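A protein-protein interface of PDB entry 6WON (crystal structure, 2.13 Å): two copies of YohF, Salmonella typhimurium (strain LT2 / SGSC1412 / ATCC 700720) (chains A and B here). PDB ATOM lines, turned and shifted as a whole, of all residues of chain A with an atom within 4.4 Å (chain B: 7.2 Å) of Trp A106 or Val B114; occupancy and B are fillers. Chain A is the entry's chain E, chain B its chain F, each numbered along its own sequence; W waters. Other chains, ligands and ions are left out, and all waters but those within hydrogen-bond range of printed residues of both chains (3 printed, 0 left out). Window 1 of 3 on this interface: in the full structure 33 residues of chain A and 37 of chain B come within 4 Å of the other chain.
NE2 of Gln B122 lies within hydrogen-bond range of O of Met A101. NE1 of Trp A106 is in hydrogen-bond range of OD1 of Asp B115, 2.9 Å away. OD2 of Asp B115 lies within salt-bridge range of NE of Arg A107, 3.5 Å away. NE of Arg B107 lies close to NH2 of Arg A107, at 3.2 Å.
Water W2 lies within hydrogen-bond range of O of Met A101 (2.7 Å), OE1 of Gln B122 (2.8 Å) and N of Phe A103 (3.0 Å). Water W3 lies within hydrogen-bond range of OD1 of Asp B115, NH2 of Arg A107 and NH2 of Arg B107. Water W1 bridges NH2 of Arg A107 and NH2 of Arg B107.
Arg B107 touches its own counterpart, Arg A107. Phe A110 touches its own counterpart, Phe B110. Positions printed for both chains: 107, 108, 109, 110 and 157. Of the 15 pairs that touch across the chains among the printed residues, 2 have their exchanged pair printed and touching as well.
Of the printed residues of chain B, Phe A103 touches Leu B66 (3.9 Å), Asp B115 (3.96 Å), Phe B118 (3.98 Å) and Leu B119 (3.6 Å). Of the printed residues of chain B, Trp A106 touches Val B114, Asp B115, Phe B118 and Leu B165. Printed residues of chain A within 4 Å of Leu B66: Phe A103. Val B114 touches just one residue of chain A: Trp A106. Of the printed residues of chain A, Ala B161 touches Phe A110 (3.9 Å) and Ala A157 (3.4 Å). The nearest residue of chain B that does not touch Trp A106 is Ala B161 (5.8 Å).
Among the printed residues, pairs that only touch across the chains: Phe A103 with Leu B66, Phe A103 with Asp B115, Phe A103 with Phe B118, Phe A103 with Leu B119, Trp A106 with Val B114, Trp A106 with Phe B118, Trp A106 with Leu B165, Phe A110 with Phe B110, Phe A110 with Ala B161, Ala A157 with Ala B161 and Ala A157 with Leu B165.
Hydrophobic or aromatic side chains of chain A within 4 Å of the printed part of chain B: Met A101, Phe A103, Trp A106, Phe A110 and Ala A157. Along chain A the printed residues that touch a printed residue of chain B span positions 101 to 157. Among the printed residues, Asp or Glu carboxylates within 4 Å of a Lys or Arg side-chain nitrogen of the other chain: Arg A107 with Asp B115 (3.5 Å).
The side-chain hydroxyl of Thr B111 lies within hydrogen-bond range of the backbone carbonyl oxygen of Arg B107, 2.9 Å away. NH2 of Arg B107 is in salt-bridge range of OD2 of Asp B115. O of Phe B110 sits at hydrogen-bond distance from N of Asp B115 (3.0 Å).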
ATOM      1  N   MET A 101     -20.815 -15.689 -27.441  1.00  0.00           N
ATOM      2  CA  MET A 101     -20.377 -14.332 -27.745  1.00  0.00           C
ATOM      3  C   MET A 101     -19.632 -13.743 -26.549  1.00  0.00           C
ATOM      4  O   MET A 101     -20.152 -13.768 -25.426  1.00  0.00           O
ATOM      5  CB  MET A 101     -21.575 -13.460 -28.108  1.00  0.00           C
ATOM      6  CG  MET A 101     -21.197 -12.098 -28.646  1.00  0.00           C
ATOM      7  SD  MET A 101     -22.576 -10.954 -28.776  1.00  0.00           S
ATOM      8  CE  MET A 101     -23.537 -11.632 -30.130  1.00  0.00           C
ATOM      9  N   PRO A 102     -18.419 -13.225 -26.739  1.00  0.00           N
ATOM     10  CA  PRO A 102     -17.703 -12.596 -25.619  1.00  0.00           C
ATOM     11  C   PRO A 102     -18.384 -11.300 -25.207  1.00  0.00           C
ATOM     12  O   PRO A 102     -18.909 -10.565 -26.044  1.00  0.00           O
ATOM     13  CB  PRO A 102     -16.305 -12.329 -26.189  1.00  0.00           C
ATOM     14  CG  PRO A 102     -16.244 -13.090 -27.479  1.00  0.00           C
ATOM     15  CD  PRO A 102     -17.640 -13.188 -27.984  1.00  0.00           C
ATOM     16  N   PHE A 103     -18.378 -11.024 -23.897  1.00  0.00           N
ATOM     17  CA  PHE A 103     -19.025  -9.811 -23.403  1.00  0.00           C
ATOM     18  C   PHE A 103     -18.426  -8.557 -24.040  1.00  0.00           C
ATOM     19  O   PHE A 103     -19.150  -7.589 -24.318  1.00  0.00           O
ATOM     20  CB  PHE A 103     -18.925  -9.747 -21.877  1.00  0.00           C
ATOM     21  CG  PHE A 103     -19.741  -8.642 -21.261  1.00  0.00           C
ATOM     22  CD1 PHE A 103     -21.117  -8.600 -21.431  1.00  0.00           C
ATOM     23  CD2 PHE A 103     -19.131  -7.647 -20.507  1.00  0.00           C
ATOM     24  CE1 PHE A 103     -21.874  -7.593 -20.861  1.00  0.00           C
ATOM     25  CE2 PHE A 103     -19.875  -6.622 -19.939  1.00  0.00           C
ATOM     26  CZ  PHE A 103     -21.246  -6.589 -20.119  1.00  0.00           C
ATOM     27  N   THR A 104     -17.108  -8.544 -24.277  1.00  0.00           N
ATOM     28  CA  THR A 104     -16.500  -7.374 -24.909  1.00  0.00           C
ATOM     29  C   THR A 104     -17.110  -7.119 -26.286  1.00  0.00           C
ATOM     30  O   THR A 104     -17.292  -5.961 -26.685  1.00  0.00           O
ATOM     31  CB  THR A 104     -14.980  -7.531 -25.029  1.00  0.00           C
ATOM     32  OG1 THR A 104     -14.679  -8.700 -25.795  1.00  0.00           O
ATOM     33  CG2 THR A 104     -14.317  -7.618 -23.654  1.00  0.00           C
ATOM     34  N   GLN A 105     -17.430  -8.188 -27.027  1.00  0.00           N
ATOM     35  CA  GLN A 105     -18.047  -8.002 -28.338  1.00  0.00           C
ATOM     36  C   GLN A 105     -19.474  -7.503 -28.199  1.00  0.00           C
ATOM     37  O   GLN A 105     -19.898  -6.613 -28.944  1.00  0.00           O
ATOM     38  CB  GLN A 105     -18.006  -9.301 -29.147  1.00  0.00           C
ATOM     39  CG  GLN A 105     -18.584  -9.174 -30.554  1.00  0.00           C
ATOM     40  CD  GLN A 105     -18.458 -10.464 -31.345  1.00  0.00           C
ATOM     41  OE1 GLN A 105     -18.513 -11.559 -30.780  1.00  0.00           O
ATOM     42  NE2 GLN A 105     -18.275 -10.342 -32.656  1.00  0.00           N
ATOM     43  N   TRP A 106     -20.229  -8.061 -27.245  1.00  0.00           N
ATOM     44  CA  TRP A 106     -21.553  -7.527 -26.934  1.00  0.00           C
ATOM     45  C   TRP A 106     -21.489  -6.025 -26.661  1.00  0.00           C
ATOM     46  O   TRP A 106     -22.248  -5.242 -27.247  1.00  0.00           O
ATOM     47  CB  TRP A 106     -22.137  -8.282 -25.740  1.00  0.00           C
ATOM     48  CG  TRP A 106     -23.402  -7.728 -25.147  1.00  0.00           C
ATOM     49  CD1 TRP A 106     -23.497  -6.829 -24.123  1.00  0.00           C
ATOM     50  CD2 TRP A 106     -24.755  -8.067 -25.510  1.00  0.00           C
ATOM     51  NE1 TRP A 106     -24.822  -6.577 -23.833  1.00  0.00           N
ATOM     52  CE2 TRP A 106     -25.613  -7.321 -24.670  1.00  0.00           C
ATOM     53  CE3 TRP A 106     -25.323  -8.917 -26.471  1.00  0.00           C
ATOM     54  CZ2 TRP A 106     -27.009  -7.404 -24.759  1.00  0.00           C
ATOM     55  CZ3 TRP A 106     -26.702  -8.997 -26.558  1.00  0.00           C
ATOM     56  CH2 TRP A 106     -27.531  -8.243 -25.708  1.00  0.00           C
ATOM     57  N   ARG A 107     -20.568  -5.603 -25.787  1.00  0.00           N
ATOM     58  CA  ARG A 107     -20.452  -4.184 -25.459  1.00  0.00           C
ATOM     59  C   ARG A 107     -20.004  -3.364 -26.666  1.00  0.00           C
ATOM     60  O   ARG A 107     -20.521  -2.265 -26.899  1.00  0.00           O
ATOM     61  CB  ARG A 107     -19.486  -3.988 -24.283  1.00  0.00           C
ATOM     62  CG  ARG A 107     -20.021  -4.506 -22.933  1.00  0.00           C
ATOM     63  CD  ARG A 107     -20.653  -3.397 -22.087  1.00  0.00           C
ATOM     64  NE  ARG A 107     -21.658  -2.627 -22.821  1.00  0.00           N
ATOM     65  CZ  ARG A 107     -21.475  -1.376 -23.242  1.00  0.00           C
ATOM     66  NH1 ARG A 107     -20.320  -0.758 -22.998  1.00  0.00           N
ATOM     67  NH2 ARG A 107     -22.438  -0.737 -23.905  1.00  0.00           N
ATOM     68  N   GLN A 108     -19.046  -3.880 -27.445  1.00  0.00           N
ATOM     69  CA  GLN A 108     -18.591  -3.161 -28.634  1.00  0.00           C
ATOM     70  C   GLN A 108     -19.750  -2.862 -29.574  1.00  0.00           C
ATOM     71  O   GLN A 108     -19.840  -1.765 -30.133  1.00  0.00           O
ATOM     72  CB  GLN A 108     -17.515  -3.965 -29.367  1.00  0.00           C
ATOM     73  CG  GLN A 108     -16.113  -3.834 -28.799  1.00  0.00           C
ATOM     74  CD  GLN A 108     -15.206  -4.985 -29.228  1.00  0.00           C
ATOM     75  OE1 GLN A 108     -15.348  -5.516 -30.334  1.00  0.00           O
ATOM     76  NE2 GLN A 108     -14.282  -5.385 -28.344  1.00  0.00           N
ATOM     77  N   ILE A 109     -20.655  -3.822 -29.752  1.00  0.00           N
ATOM     78  CA  ILE A 109     -21.753  -3.624 -30.693  1.00  0.00           C
ATOM     79  C   ILE A 109     -22.736  -2.589 -30.161  1.00  0.00           C
ATOM     80  O   ILE A 109     -23.190  -1.709 -30.906  1.00  0.00           O
ATOM     81  CB  ILE A 109     -22.427  -4.973 -30.998  1.00  0.00           C
ATOM     82  CG1 ILE A 109     -21.499  -5.828 -31.877  1.00  0.00           C
ATOM     83  CG2 ILE A 109     -23.761  -4.768 -31.674  1.00  0.00           C
ATOM     84  CD1 ILE A 109     -21.591  -7.322 -31.600  1.00  0.00           C
ATOM     85  N   PHE A 110     -23.061  -2.654 -28.864  1.00  0.00           N
ATOM     86  CA  PHE A 110     -23.914  -1.628 -28.266  1.00  0.00           C
ATOM     87  C   PHE A 110     -23.250  -0.252 -28.297  1.00  0.00           C
ATOM     88  O   PHE A 110     -23.930   0.768 -28.495  1.00  0.00           O
ATOM     89  CB  PHE A 110     -24.275  -2.018 -26.835  1.00  0.00           C
ATOM     90  CG  PHE A 110     -25.548  -2.814 -26.743  1.00  0.00           C
ATOM     91  CD1 PHE A 110     -25.550  -4.171 -27.029  1.00  0.00           C
ATOM     92  CD2 PHE A 110     -26.739  -2.195 -26.410  1.00  0.00           C
ATOM     93  CE1 PHE A 110     -26.702  -4.894 -26.983  1.00  0.00           C
ATOM     94  CE2 PHE A 110     -27.911  -2.918 -26.350  1.00  0.00           C
ATOM     95  CZ  PHE A 110     -27.896  -4.272 -26.644  1.00  0.00           C
ATOM     96  N   ALA A 154     -26.785  -9.537 -30.710  1.00  0.00           N
ATOM     97  CA  ALA A 154     -26.386  -8.217 -30.236  1.00  0.00           C
ATOM     98  C   ALA A 154     -26.870  -7.129 -31.188  1.00  0.00           C
ATOM     99  O   ALA A 154     -27.367  -6.080 -30.750  1.00  0.00           O
ATOM    100  CB  ALA A 154     -24.869  -8.152 -30.062  1.00  0.00           C
ATOM    101  N   ALA A 157     -30.555  -6.691 -30.686  1.00  0.00           N
ATOM    102  CA  ALA A 157     -30.886  -6.048 -29.418  1.00  0.00           C
ATOM    103  C   ALA A 157     -30.576  -4.561 -29.468  1.00  0.00           C
ATOM    104  O   ALA A 157     -31.341  -3.745 -28.949  1.00  0.00           O
ATOM    105  CB  ALA A 157     -30.137  -6.723 -28.261  1.00  0.00           C
ATOM    106  N   LEU B  66     -19.647  -6.191 -14.364  1.00  0.00           N
ATOM    107  CA  LEU B  66     -19.655  -7.360 -15.230  1.00  0.00           C
ATOM    108  C   LEU B  66     -18.350  -7.475 -16.007  1.00  0.00           C
ATOM    109  O   LEU B  66     -17.607  -6.495 -16.134  1.00  0.00           O
ATOM    110  CB  LEU B  66     -20.839  -7.261 -16.200  1.00  0.00           C
ATOM    111  CG  LEU B  66     -22.153  -6.974 -15.476  1.00  0.00           C
ATOM    112  CD1 LEU B  66     -23.309  -6.894 -16.450  1.00  0.00           C
ATOM    113  CD2 LEU B  66     -22.410  -8.049 -14.401  1.00  0.00           C
ATOM    114  N   ASN B  88     -35.022 -13.832 -15.667  1.00  0.00           N
ATOM    115  CA  ASN B  88     -34.210 -12.616 -15.634  1.00  0.00           C
ATOM    116  C   ASN B  88     -35.082 -11.486 -15.108  1.00  0.00           C
ATOM    117  O   ASN B  88     -35.886 -10.916 -15.846  1.00  0.00           O
ATOM    118  CB  ASN B  88     -33.674 -12.283 -17.021  1.00  0.00           C
ATOM    119  CG  ASN B  88     -32.318 -12.887 -17.281  1.00  0.00           C
ATOM    120  OD1 ASN B  88     -31.485 -12.988 -16.371  1.00  0.00           O
ATOM    121  ND2 ASN B  88     -32.076 -13.291 -18.533  1.00  0.00           N
ATOM    122  N   ARG B 107     -24.962   4.059 -19.043  1.00  0.00           N
ATOM    123  CA  ARG B 107     -24.292   2.762 -19.024  1.00  0.00           C
ATOM    124  C   ARG B 107     -24.735   1.924 -17.829  1.00  0.00           C
ATOM    125  O   ARG B 107     -24.937   0.712 -17.960  1.00  0.00           O
ATOM    126  CB  ARG B 107     -22.772   2.955 -19.021  1.00  0.00           C
ATOM    127  CG  ARG B 107     -22.182   3.382 -20.381  1.00  0.00           C
ATOM    128  CD  ARG B 107     -21.732   2.176 -21.225  1.00  0.00           C
ATOM    129  NE  ARG B 107     -22.788   1.171 -21.395  1.00  0.00           N
ATOM    130  CZ  ARG B 107     -22.821   0.002 -20.751  1.00  0.00           C
ATOM    131  NH1 ARG B 107     -21.846  -0.319 -19.901  1.00  0.00           N
ATOM    132  NH2 ARG B 107     -23.818  -0.856 -20.964  1.00  0.00           N
ATOM    133  N   GLN B 108     -24.888   2.547 -16.651  1.00  0.00           N
ATOM    134  CA  GLN B 108     -25.314   1.793 -15.474  1.00  0.00           C
ATOM    135  C   GLN B 108     -26.693   1.189 -15.682  1.00  0.00           C
ATOM    136  O   GLN B 108     -26.946   0.045 -15.280  1.00  0.00           O
ATOM    137  CB  GLN B 108     -25.308   2.682 -14.229  1.00  0.00           C
ATOM    138  CG  GLN B 108     -23.899   3.077 -13.795  1.00  0.00           C
ATOM    139  CD  GLN B 108     -23.851   3.932 -12.528  1.00  0.00           C
ATOM    140  OE1 GLN B 108     -23.334   3.509 -11.490  1.00  0.00           O
ATOM    141  NE2 GLN B 108     -24.387   5.145 -12.616  1.00  0.00           N
ATOM    142  N   ILE B 109     -27.593   1.937 -16.321  1.00  0.00           N
ATOM    143  CA  ILE B 109     -28.943   1.438 -16.549  1.00  0.00           C
ATOM    144  C   ILE B 109     -28.927   0.278 -17.537  1.00  0.00           C
ATOM    145  O   ILE B 109     -29.620  -0.727 -17.342  1.00  0.00           O
ATOM    146  CB  ILE B 109     -29.859   2.590 -17.000  1.00  0.00           C
ATOM    147  CG1 ILE B 109     -30.108   3.538 -15.825  1.00  0.00           C
ATOM    148  CG2 ILE B 109     -31.196   2.054 -17.538  1.00  0.00           C
ATOM    149  CD1 ILE B 109     -30.837   4.806 -16.194  1.00  0.00           C
ATOM    150  N   PHE B 110     -28.119   0.375 -18.598  1.00  0.00           N
ATOM    151  CA  PHE B 110     -28.006  -0.760 -19.519  1.00  0.00           C
ATOM    152  C   PHE B 110     -27.350  -1.952 -18.835  1.00  0.00           C
ATOM    153  O   PHE B 110     -27.735  -3.105 -19.072  1.00  0.00           O
ATOM    154  CB  PHE B 110     -27.220  -0.366 -20.774  1.00  0.00           C
ATOM    155  CG  PHE B 110     -28.089   0.140 -21.890  1.00  0.00           C
ATOM    156  CD1 PHE B 110     -28.666   1.404 -21.817  1.00  0.00           C
ATOM    157  CD2 PHE B 110     -28.369  -0.663 -22.996  1.00  0.00           C
ATOM    158  CE1 PHE B 110     -29.484   1.871 -22.844  1.00  0.00           C
ATOM    159  CE2 PHE B 110     -29.190  -0.205 -24.026  1.00  0.00           C
ATOM    160  CZ  PHE B 110     -29.747   1.066 -23.951  1.00  0.00           C
ATOM    161  N   THR B 111     -26.353  -1.687 -17.986  1.00  0.00           N
ATOM    162  CA  THR B 111     -25.659  -2.749 -17.266  1.00  0.00           C
ATOM    163  C   THR B 111     -26.634  -3.626 -16.493  1.00  0.00           C
ATOM    164  O   THR B 111     -26.578  -4.858 -16.578  1.00  0.00           O
ATOM    165  CB  THR B 111     -24.620  -2.137 -16.325  1.00  0.00           C
ATOM    166  OG1 THR B 111     -23.518  -1.656 -17.098  1.00  0.00           O
ATOM    167  CG2 THR B 111     -24.110  -3.167 -15.313  1.00  0.00           C
ATOM    168  N   VAL B 112     -27.551  -3.006 -15.749  1.00  0.00           N
ATOM    169  CA  VAL B 112     -28.451  -3.767 -14.890  1.00  0.00           C
ATOM    170  C   VAL B 112     -29.719  -4.240 -15.594  1.00  0.00           C
ATOM    171  O   VAL B 112     -30.372  -5.172 -15.104  1.00  0.00           O
ATOM    172  CB  VAL B 112     -28.848  -2.950 -13.648  1.00  0.00           C
ATOM    173  CG1 VAL B 112     -27.637  -2.728 -12.747  1.00  0.00           C
ATOM    174  CG2 VAL B 112     -29.487  -1.634 -14.056  1.00  0.00           C
ATOM    175  N   ASP B 113     -30.080  -3.647 -16.729  1.00  0.00           N
ATOM    176  CA  ASP B 113     -31.346  -3.938 -17.354  1.00  0.00           C
ATOM    177  C   ASP B 113     -31.220  -4.877 -18.577  1.00  0.00           C
ATOM    178  O   ASP B 113     -32.215  -5.508 -18.942  1.00  0.00           O
ATOM    179  CB  ASP B 113     -32.093  -2.660 -17.715  1.00  0.00           C
ATOM    180  CG  ASP B 113     -32.916  -2.147 -16.555  1.00  0.00           C
ATOM    181  OD1 ASP B 113     -33.522  -2.995 -15.860  1.00  0.00           O
ATOM    182  OD2 ASP B 113     -32.961  -0.912 -16.336  1.00  0.00           O
ATOM    183  N   VAL B 114     -30.051  -4.965 -19.215  1.00  0.00           N
ATOM    184  CA  VAL B 114     -29.900  -5.911 -20.286  1.00  0.00           C
ATOM    185  C   VAL B 114     -28.564  -6.660 -20.302  1.00  0.00           C
ATOM    186  O   VAL B 114     -28.504  -7.836 -20.671  1.00  0.00           O
ATOM    187  CB  VAL B 114     -30.139  -5.189 -21.641  1.00  0.00           C
ATOM    188  CG1 VAL B 114     -29.065  -4.167 -21.919  1.00  0.00           C
ATOM    189  CG2 VAL B 114     -30.224  -6.188 -22.792  1.00  0.00           C
ATOM    190  N   ASP B 115     -27.481  -5.993 -19.891  1.00  0.00           N
ATOM    191  CA  ASP B 115     -26.183  -6.664 -19.878  1.00  0.00           C
ATOM    192  C   ASP B 115     -26.183  -7.838 -18.900  1.00  0.00           C
ATOM    193  O   ASP B 115     -25.725  -8.938 -19.229  1.00  0.00           O
ATOM    194  CB  ASP B 115     -25.072  -5.668 -19.530  1.00  0.00           C
ATOM    195  CG  ASP B 115     -24.829  -4.640 -20.642  1.00  0.00           C
ATOM    196  OD1 ASP B 115     -25.485  -4.729 -21.714  1.00  0.00           O
ATOM    197  OD2 ASP B 115     -23.979  -3.743 -20.431  1.00  0.00           O
ATOM    198  N   GLY B 116     -26.692  -7.623 -17.687  1.00  0.00           N
ATOM    199  CA  GLY B 116     -26.766  -8.715 -16.730  1.00  0.00           C
ATOM    200  C   GLY B 116     -27.656  -9.844 -17.212  1.00  0.00           C
ATOM    201  O   GLY B 116     -27.303 -11.024 -17.107  1.00  0.00           O
ATOM    202  N   ALA B 117     -28.823  -9.498 -17.757  1.00  0.00           N
ATOM    203  CA  ALA B 117     -29.705 -10.527 -18.303  1.00  0.00           C
ATOM    204  C   ALA B 117     -29.013 -11.309 -19.412  1.00  0.00           C
ATOM    205  O   ALA B 117     -29.101 -12.541 -19.459  1.00  0.00           O
ATOM    206  CB  ALA B 117     -31.002  -9.901 -18.810  1.00  0.00           C
ATOM    207  N   PHE B 118     -28.285 -10.614 -20.292  1.00  0.00           N
ATOM    208  CA  PHE B 118     -27.589 -11.298 -21.378  1.00  0.00           C
ATOM    209  C   PHE B 118     -26.568 -12.303 -20.837  1.00  0.00           C
ATOM    210  O   PHE B 118     -26.540 -13.465 -21.262  1.00  0.00           O
ATOM    211  CB  PHE B 118     -26.925 -10.273 -22.303  1.00  0.00           C
ATOM    212  CG  PHE B 118     -25.796 -10.837 -23.118  1.00  0.00           C
ATOM    213  CD1 PHE B 118     -26.042 -11.777 -24.110  1.00  0.00           C
ATOM    214  CD2 PHE B 118     -24.484 -10.443 -22.884  1.00  0.00           C
ATOM    215  CE1 PHE B 118     -25.009 -12.310 -24.857  1.00  0.00           C
ATOM    216  CE2 PHE B 118     -23.438 -10.970 -23.635  1.00  0.00           C
ATOM    217  CZ  PHE B 118     -23.698 -11.900 -24.625  1.00  0.00           C
ATOM    218  N   LEU B 119     -25.747 -11.892 -19.867  1.00  0.00           N
ATOM    219  CA  LEU B 119     -24.730 -12.811 -19.348  1.00  0.00           C
ATOM    220  C   LEU B 119     -25.355 -13.950 -18.549  1.00  0.00           C
ATOM    221  O   LEU B 119     -24.859 -15.084 -18.589  1.00  0.00           O
ATOM    222  CB  LEU B 119     -23.721 -12.061 -18.485  1.00  0.00           C
ATOM    223  CG  LEU B 119     -22.774 -11.096 -19.197  1.00  0.00           C
ATOM    224  CD1 LEU B 119     -22.037 -10.244 -18.174  1.00  0.00           C
ATOM    225  CD2 LEU B 119     -21.791 -11.838 -20.096  1.00  0.00           C
ATOM    226  N   CYS B 120     -26.434 -13.674 -17.812  1.00  0.00           N
ATOM    227  CA  CYS B 120     -27.074 -14.738 -17.043  1.00  0.00           C
ATOM    228  C   CYS B 120     -27.744 -15.749 -17.963  1.00  0.00           C
ATOM    229  O   CYS B 120     -27.660 -16.960 -17.725  1.00  0.00           O
ATOM    230  CB  CYS B 120     -28.094 -14.159 -16.061  1.00  0.00           C
ATOM    231  SG  CYS B 120     -27.379 -13.188 -14.709  1.00  0.00           S
ATOM    232  N   GLN B 122     -26.908 -16.475 -21.058  1.00  0.00           N
ATOM    233  CA  GLN B 122     -25.838 -17.264 -21.660  1.00  0.00           C
ATOM    234  C   GLN B 122     -25.452 -18.441 -20.768  1.00  0.00           C
ATOM    235  O   GLN B 122     -25.392 -19.590 -21.219  1.00  0.00           O
ATOM    236  CB  GLN B 122     -24.617 -16.376 -21.905  1.00  0.00           C
ATOM    237  CG  GLN B 122     -24.446 -15.912 -23.322  1.00  0.00           C
ATOM    238  CD  GLN B 122     -23.110 -15.241 -23.530  1.00  0.00           C
ATOM    239  OE1 GLN B 122     -22.563 -14.640 -22.603  1.00  0.00           O
ATOM    240  NE2 GLN B 122     -22.564 -15.347 -24.746  1.00  0.00           N
ATOM    241  N   ALA B 157     -34.926   2.365 -23.487  1.00  0.00           N
ATOM    242  CA  ALA B 157     -34.025   1.798 -24.488  1.00  0.00           C
ATOM    243  C   ALA B 157     -33.550   0.410 -24.079  1.00  0.00           C
ATOM    244  O   ALA B 157     -33.522  -0.513 -24.903  1.00  0.00           O
ATOM    245  CB  ALA B 157     -32.832   2.730 -24.711  1.00  0.00           C
ATOM    246  N   ALA B 158     -33.191   0.241 -22.802  1.00  0.00           N
ATOM    247  CA  ALA B 158     -32.656  -1.036 -22.333  1.00  0.00           C
ATOM    248  C   ALA B 158     -33.730  -2.117 -22.316  1.00  0.00           C
ATOM    249  O   ALA B 158     -33.441  -3.283 -22.619  1.00  0.00           O
ATOM    250  CB  ALA B 158     -32.038  -0.867 -20.945  1.00  0.00           C
ATOM    251  N   LYS B 159     -34.975  -1.754 -21.956  1.00  0.00           N
ATOM    252  CA  LYS B 159     -36.075  -2.716 -22.008  1.00  0.00           C
ATOM    253  C   LYS B 159     -36.367  -3.137 -23.439  1.00  0.00           C
ATOM    254  O   LYS B 159     -36.676  -4.307 -23.700  1.00  0.00           O
ATOM    255  CB  LYS B 159     -37.337  -2.122 -21.380  1.00  0.00           C
ATOM    256  CG  LYS B 159     -37.194  -1.830 -19.900  1.00  0.00           C
ATOM    257  CD  LYS B 159     -36.869  -3.095 -19.119  1.00  0.00           C
ATOM    258  CE  LYS B 159     -37.492  -3.038 -17.749  1.00  0.00           C
ATOM    259  NZ  LYS B 159     -36.896  -4.016 -16.838  1.00  0.00           N
ATOM    260  N   HIS B 160     -36.325  -2.182 -24.373  1.00  0.00           N
ATOM    261  CA  HIS B 160     -36.430  -2.529 -25.785  1.00  0.00           C
ATOM    262  C   HIS B 160     -35.314  -3.495 -26.174  1.00  0.00           C
ATOM    263  O   HIS B 160     -35.549  -4.478 -26.889  1.00  0.00           O
ATOM    264  CB  HIS B 160     -36.366  -1.264 -26.649  1.00  0.00           C
ATOM    265  CG  HIS B 160     -37.672  -0.539 -26.782  1.00  0.00           C
ATOM    266  ND1 HIS B 160     -38.316   0.051 -25.714  1.00  0.00           N
ATOM    267  CD2 HIS B 160     -38.436  -0.275 -27.875  1.00  0.00           C
ATOM    268  CE1 HIS B 160     -39.429   0.628 -26.138  1.00  0.00           C
ATOM    269  NE2 HIS B 160     -39.528   0.445 -27.446  1.00  0.00           N
ATOM    270  N   ALA B 161     -34.092  -3.243 -25.686  1.00  0.00           N
ATOM    271  CA  ALA B 161     -32.981  -4.130 -26.008  1.00  0.00           C
ATOM    272  C   ALA B 161     -33.257  -5.539 -25.519  1.00  0.00           C
ATOM    273  O   ALA B 161     -33.012  -6.515 -26.237  1.00  0.00           O
ATOM    274  CB  ALA B 161     -31.675  -3.595 -25.409  1.00  0.00           C
ATOM    275  N   LEU B 162     -33.795  -5.663 -24.307  1.00  0.00           N
ATOM    276  CA  LEU B 162     -34.055  -6.977 -23.733  1.00  0.00           C
ATOM    277  C   LEU B 162     -35.189  -7.698 -24.462  1.00  0.00           C
ATOM    278  O   LEU B 162     -35.180  -8.932 -24.555  1.00  0.00           O
ATOM    279  CB  LEU B 162     -34.368  -6.823 -22.242  1.00  0.00           C
ATOM    280  CG  LEU B 162     -34.559  -8.083 -21.381  1.00  0.00           C
ATOM    281  CD1 LEU B 162     -33.462  -9.140 -21.626  1.00  0.00           C
ATOM    282  CD2 LEU B 162     -34.620  -7.686 -19.888  1.00  0.00           C
ATOM    283  N   GLY B 163     -36.172  -6.953 -24.967  1.00  0.00           N
ATOM    284  CA  GLY B 163     -37.181  -7.555 -25.831  1.00  0.00           C
ATOM    285  C   GLY B 163     -36.605  -8.085 -27.135  1.00  0.00           C
ATOM    286  O   GLY B 163     -37.000  -9.157 -27.608  1.00  0.00           O
ATOM    287  N   LEU B 165     -33.313  -9.006 -27.618  1.00  0.00           N
ATOM    288  CA  LEU B 165     -32.566 -10.188 -27.211  1.00  0.00           C
ATOM    289  C   LEU B 165     -33.504 -11.382 -27.007  1.00  0.00           C
ATOM    290  O   LEU B 165     -33.173 -12.517 -27.373  1.00  0.00           O
ATOM    291  CB  LEU B 165     -31.780  -9.882 -25.928  1.00  0.00           C
ATOM    292  CG  LEU B 165     -30.962 -11.042 -25.365  1.00  0.00           C
ATOM    293  CD1 LEU B 165     -30.020 -11.552 -26.458  1.00  0.00           C
ATOM    294  CD2 LEU B 165     -30.194 -10.624 -24.090  1.00  0.00           C
HETATM  295  O   HOH W   1     -25.147   0.542 -23.492  1.00  0.00           O
HETATM  296  O   HOH W   2     -20.227 -13.164 -22.810  1.00  0.00           O
HETATM  297  O   HOH W   3     -24.650  -2.705 -23.439  1.00  0.00           O
